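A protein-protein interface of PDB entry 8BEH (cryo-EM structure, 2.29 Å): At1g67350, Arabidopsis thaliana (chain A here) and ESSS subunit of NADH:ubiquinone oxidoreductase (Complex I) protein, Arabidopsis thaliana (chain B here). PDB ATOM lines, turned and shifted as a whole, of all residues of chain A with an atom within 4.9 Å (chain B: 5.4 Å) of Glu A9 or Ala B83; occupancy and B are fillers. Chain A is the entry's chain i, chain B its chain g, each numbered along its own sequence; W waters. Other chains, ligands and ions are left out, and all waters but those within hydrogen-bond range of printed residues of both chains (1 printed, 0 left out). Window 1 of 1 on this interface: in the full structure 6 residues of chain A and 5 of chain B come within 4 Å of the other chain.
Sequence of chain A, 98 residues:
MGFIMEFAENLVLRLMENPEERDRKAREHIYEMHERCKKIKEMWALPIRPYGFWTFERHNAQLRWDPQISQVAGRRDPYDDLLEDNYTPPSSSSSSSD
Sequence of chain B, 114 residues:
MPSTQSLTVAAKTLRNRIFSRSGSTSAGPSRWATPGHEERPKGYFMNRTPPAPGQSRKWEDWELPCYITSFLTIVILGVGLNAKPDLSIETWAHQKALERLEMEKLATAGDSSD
The backbone carbonyl oxygen (O) of Ala B83 sits close to the side-chain carboxylate (OE2) of Glu A9 (2.8 Å).
The backbone carbonyl oxygen (O) of Met A5 lies close to the side-chain carboxylate (OE1) of Glu A9.
Among the printed residues, pairs that only touch across the chains: Met A5 with Val B79, Met A5 with Asn B82, Met A5 with Ala B83, Ala A8 with Val B79, Ala A8 with Ala B83, Glu A9 with Asn B82, Val A12 with Lys B84, Val A12 with Pro B85 and Leu A13 with Pro B85.
Phe A7 touches none of the printed residues of chain B.
Of chain B, only Asn B82 (3.8 Å) and Ala B83 (2.8 Å) come within 4 Å of Glu A9.
Leu A11 touches none of the printed residues of chain B.
Printed residues of chain B within 4 Å of Leu A13: Pro B85.
Of the printed residues of chain A, Asn B82 touches Met A5 (3.4 Å) and Glu A9 (3.8 Å).
Ala B83 touches just these residues of chain A: Met A5, Ala A8 and Glu A9.
Of the printed residues of chain A, Lys B84 touches Val A12.
Of the printed residues of chain A, Pro B85 touches Val A12 and Leu A13.
The nearest residue of chain A that does not touch Ala B83 is Val A12 (4.4 Å).
Printed residues of chain B that touch a printed residue of chain A: Val B79, Asn B82, Ala B83, Lys B84 and Pro B85.
Hydrophobic or aromatic side chains of chain B within 4 Å of the printed part of chain A: Val B79, Ala B83 and Pro B85.
Printed residues of chain A that touch a printed residue of chain B: Met A5, Ala A8, Glu A9, Val A12 and Leu A13.
Hydrophobic or aromatic side chains of chain A within 4 Å of the printed part of chain B: Met A5, Ala A8, Val A12 and Leu A13.
Water W1 bridges the backbone carbonyl oxygen of Glu A9 (2.8 Å) and the backbone carbonyl oxygen of Ala B83 (3.0 Å).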
ATOM      1  N   MET A   5     -11.054 -31.528  26.816  1.00  0.00           N
ATOM      2  CA  MET A   5     -12.426 -31.358  27.247  1.00  0.00           C
ATOM      3  C   MET A   5     -12.492 -30.846  28.684  1.00  0.00           C
ATOM      4  O   MET A   5     -13.279 -29.949  28.887  1.00  0.00           O
ATOM      5  CB  MET A   5     -13.236 -32.623  26.974  1.00  0.00           C
ATOM      6  CG  MET A   5     -14.543 -32.333  26.271  1.00  0.00           C
ATOM      7  SD  MET A   5     -14.337 -31.737  24.561  1.00  0.00           S
ATOM      8  CE  MET A   5     -16.031 -31.323  24.183  1.00  0.00           C
ATOM      9  N   GLU A   6     -11.660 -31.325  29.606  1.00  0.00           N
ATOM     10  CA  GLU A   6     -11.820 -30.853  30.996  1.00  0.00           C
ATOM     11  C   GLU A   6     -11.568 -29.338  31.003  1.00  0.00           C
ATOM     12  O   GLU A   6     -12.394 -28.628  31.565  1.00  0.00           O
ATOM     13  CB  GLU A   6     -11.002 -31.680  31.990  1.00  0.00           C
ATOM     14  CG  GLU A   6     -11.107 -31.165  33.411  1.00  0.00           C
ATOM     15  CD  GLU A   6      -9.928 -31.504  34.305  1.00  0.00           C
ATOM     16  OE1 GLU A   6      -8.870 -31.889  33.766  1.00  0.00           O
ATOM     17  OE2 GLU A   6     -10.069 -31.376  35.537  1.00  0.00           O
ATOM     18  N   PHE A   7     -10.551 -28.889  30.295  1.00  0.00           N
ATOM     19  CA  PHE A   7     -10.289 -27.437  30.177  1.00  0.00           C
ATOM     20  C   PHE A   7     -11.538 -26.786  29.568  1.00  0.00           C
ATOM     21  O   PHE A   7     -11.915 -25.761  30.045  1.00  0.00           O
ATOM     22  CB  PHE A   7      -8.977 -27.188  29.415  1.00  0.00           C
ATOM     23  CG  PHE A   7      -8.814 -25.781  28.922  1.00  0.00           C
ATOM     24  CD1 PHE A   7      -9.407 -25.373  27.740  1.00  0.00           C
ATOM     25  CD2 PHE A   7      -8.109 -24.858  29.666  1.00  0.00           C
ATOM     26  CE1 PHE A   7      -9.282 -24.067  27.308  1.00  0.00           C
ATOM     27  CE2 PHE A   7      -7.982 -23.556  29.230  1.00  0.00           C
ATOM     28  CZ  PHE A   7      -8.564 -23.163  28.051  1.00  0.00           C
ATOM     29  N   ALA A   8     -12.086 -27.387  28.508  1.00  0.00           N
ATOM     30  CA  ALA A   8     -13.253 -26.789  27.867  1.00  0.00           C
ATOM     31  C   ALA A   8     -14.441 -26.714  28.825  1.00  0.00           C
ATOM     32  O   ALA A   8     -15.170 -25.715  28.835  1.00  0.00           O
ATOM     33  CB  ALA A   8     -13.613 -27.568  26.606  1.00  0.00           C
ATOM     34  N   GLU A   9     -14.653 -27.762  29.629  1.00  0.00           N
ATOM     35  CA  GLU A   9     -15.678 -27.718  30.672  1.00  0.00           C
ATOM     36  C   GLU A   9     -15.489 -26.503  31.561  1.00  0.00           C
ATOM     37  O   GLU A   9     -16.421 -25.720  31.787  1.00  0.00           O
ATOM     38  CB  GLU A   9     -15.641 -28.966  31.560  1.00  0.00           C
ATOM     39  CG  GLU A   9     -16.505 -30.177  31.240  1.00  0.00           C
ATOM     40  CD  GLU A   9     -16.279 -30.816  29.898  1.00  0.00           C
ATOM     41  OE1 GLU A   9     -15.275 -31.536  29.745  1.00  0.00           O
ATOM     42  OE2 GLU A   9     -17.146 -30.686  29.028  1.00  0.00           O
ATOM     43  N   ASN A  10     -14.274 -26.342  32.080  1.00  0.00           N
ATOM     44  CA  ASN A  10     -14.011 -25.252  33.010  1.00  0.00           C
ATOM     45  C   ASN A  10     -14.187 -23.895  32.342  1.00  0.00           C
ATOM     46  O   ASN A  10     -14.752 -22.973  32.938  1.00  0.00           O
ATOM     47  CB  ASN A  10     -12.613 -25.400  33.603  1.00  0.00           C
ATOM     48  CG  ASN A  10     -12.529 -26.535  34.590  1.00  0.00           C
ATOM     49  OD1 ASN A  10     -13.538 -27.154  34.922  1.00  0.00           O
ATOM     50  ND2 ASN A  10     -11.322 -26.820  35.069  1.00  0.00           N
ATOM     51  N   LEU A  11     -13.719 -23.759  31.103  1.00  0.00           N
ATOM     52  CA  LEU A  11     -13.846 -22.489  30.395  1.00  0.00           C
ATOM     53  C   LEU A  11     -15.310 -22.128  30.166  1.00  0.00           C
ATOM     54  O   LEU A  11     -15.724 -20.982  30.389  1.00  0.00           O
ATOM     55  CB  LEU A  11     -13.083 -22.564  29.074  1.00  0.00           C
ATOM     56  CG  LEU A  11     -13.106 -21.347  28.156  1.00  0.00           C
ATOM     57  CD1 LEU A  11     -12.828 -20.070  28.936  1.00  0.00           C
ATOM     58  CD2 LEU A  11     -12.114 -21.532  27.036  1.00  0.00           C
ATOM     59  N   VAL A  12     -16.117 -23.100  29.731  1.00  0.00           N
ATOM     60  CA  VAL A  12     -17.540 -22.845  29.526  1.00  0.00           C
ATOM     61  C   VAL A  12     -18.199 -22.444  30.838  1.00  0.00           C
ATOM     62  O   VAL A  12     -19.005 -21.506  30.883  1.00  0.00           O
ATOM     63  CB  VAL A  12     -18.229 -24.071  28.898  1.00  0.00           C
ATOM     64  CG1 VAL A  12     -19.739 -23.915  28.967  1.00  0.00           C
ATOM     65  CG2 VAL A  12     -17.787 -24.259  27.460  1.00  0.00           C
ATOM     66  N   LEU A  13     -17.863 -23.142  31.927  1.00  0.00           N
ATOM     67  CA  LEU A  13     -18.413 -22.778  33.229  1.00  0.00           C
ATOM     68  C   LEU A  13     -18.028 -21.351  33.604  1.00  0.00           C
ATOM     69  O   LEU A  13     -18.841 -20.604  34.160  1.00  0.00           O
ATOM     70  CB  LEU A  13     -17.930 -23.761  34.293  1.00  0.00           C
ATOM     71  CG  LEU A  13     -18.542 -25.162  34.327  1.00  0.00           C
ATOM     72  CD1 LEU A  13     -18.268 -25.808  35.665  1.00  0.00           C
ATOM     73  CD2 LEU A  13     -20.033 -25.136  34.032  1.00  0.00           C
ATOM     74  N   VAL B  79     -16.664 -28.404  20.151  1.00  0.00           N
ATOM     75  CA  VAL B  79     -16.092 -28.495  21.486  1.00  0.00           C
ATOM     76  C   VAL B  79     -17.038 -27.924  22.534  1.00  0.00           C
ATOM     77  O   VAL B  79     -17.349 -28.592  23.520  1.00  0.00           O
ATOM     78  CB  VAL B  79     -14.710 -27.807  21.526  1.00  0.00           C
ATOM     79  CG1 VAL B  79     -14.179 -27.767  22.947  1.00  0.00           C
ATOM     80  CG2 VAL B  79     -13.736 -28.523  20.608  1.00  0.00           C
ATOM     81  N   GLY B  80     -17.520 -26.691  22.345  1.00  0.00           N
ATOM     82  CA  GLY B  80     -18.354 -26.067  23.356  1.00  0.00           C
ATOM     83  C   GLY B  80     -19.683 -26.765  23.567  1.00  0.00           C
ATOM     84  O   GLY B  80     -20.159 -26.865  24.700  1.00  0.00           O
ATOM     85  N   LEU B  81     -20.312 -27.240  22.489  1.00  0.00           N
ATOM     86  CA  LEU B  81     -21.585 -27.933  22.648  1.00  0.00           C
ATOM     87  C   LEU B  81     -21.420 -29.233  23.425  1.00  0.00           C
ATOM     88  O   LEU B  81     -22.252 -29.548  24.280  1.00  0.00           O
ATOM     89  CB  LEU B  81     -22.226 -28.197  21.286  1.00  0.00           C
ATOM     90  CG  LEU B  81     -22.841 -26.981  20.579  1.00  0.00           C
ATOM     91  CD1 LEU B  81     -23.483 -27.384  19.265  1.00  0.00           C
ATOM     92  CD2 LEU B  81     -23.836 -26.253  21.463  1.00  0.00           C
ATOM     93  N   ASN B  82     -20.355 -29.987  23.160  1.00  0.00           N
ATOM     94  CA  ASN B  82     -20.064 -31.187  23.930  1.00  0.00           C
ATOM     95  C   ASN B  82     -19.393 -30.894  25.262  1.00  0.00           C
ATOM     96  O   ASN B  82     -19.280 -31.801  26.089  1.00  0.00           O
ATOM     97  CB  ASN B  82     -19.180 -32.147  23.130  1.00  0.00           C
ATOM     98  CG  ASN B  82     -19.862 -32.672  21.896  1.00  0.00           C
ATOM     99  OD1 ASN B  82     -20.733 -33.534  21.969  1.00  0.00           O
ATOM    100  ND2 ASN B  82     -19.465 -32.157  20.746  1.00  0.00           N
ATOM    101  N   ALA B  83     -18.955 -29.657  25.498  1.00  0.00           N
ATOM    102  CA  ALA B  83     -18.312 -29.312  26.755  1.00  0.00           C
ATOM    103  C   ALA B  83     -19.203 -28.544  27.716  1.00  0.00           C
ATOM    104  O   ALA B  83     -18.931 -28.549  28.919  1.00  0.00           O
ATOM    105  CB  ALA B  83     -17.038 -28.492  26.516  1.00  0.00           C
ATOM    106  N   LYS B  84     -20.240 -27.883  27.225  1.00  0.00           N
ATOM    107  CA  LYS B  84     -21.130 -27.155  28.104  1.00  0.00           C
ATOM    108  C   LYS B  84     -21.946 -28.127  28.957  1.00  0.00           C
ATOM    109  O   LYS B  84     -22.280 -29.228  28.512  1.00  0.00           O
ATOM    110  CB  LYS B  84     -22.043 -26.244  27.290  1.00  0.00           C
ATOM    111  CG  LYS B  84     -23.137 -26.956  26.528  1.00  0.00           C
ATOM    112  CD  LYS B  84     -24.021 -25.976  25.784  1.00  0.00           C
ATOM    113  CE  LYS B  84     -24.261 -24.708  26.588  1.00  0.00           C
ATOM    114  NZ  LYS B  84     -25.532 -24.042  26.202  1.00  0.00           N
ATOM    115  N   PRO B  85     -22.253 -27.752  30.197  1.00  0.00           N
ATOM    116  CA  PRO B  85     -23.026 -28.646  31.063  1.00  0.00           C
ATOM    117  C   PRO B  85     -24.419 -28.884  30.502  1.00  0.00           C
ATOM    118  O   PRO B  85     -25.010 -28.017  29.856  1.00  0.00           O
ATOM    119  CB  PRO B  85     -23.084 -27.887  32.392  1.00  0.00           C
ATOM    120  CG  PRO B  85     -22.933 -26.459  32.008  1.00  0.00           C
ATOM    121  CD  PRO B  85     -22.010 -26.445  30.828  1.00  0.00           C
HETATM  122  O   HOH W   1     -18.886 -26.901  31.390  1.00  0.00           O
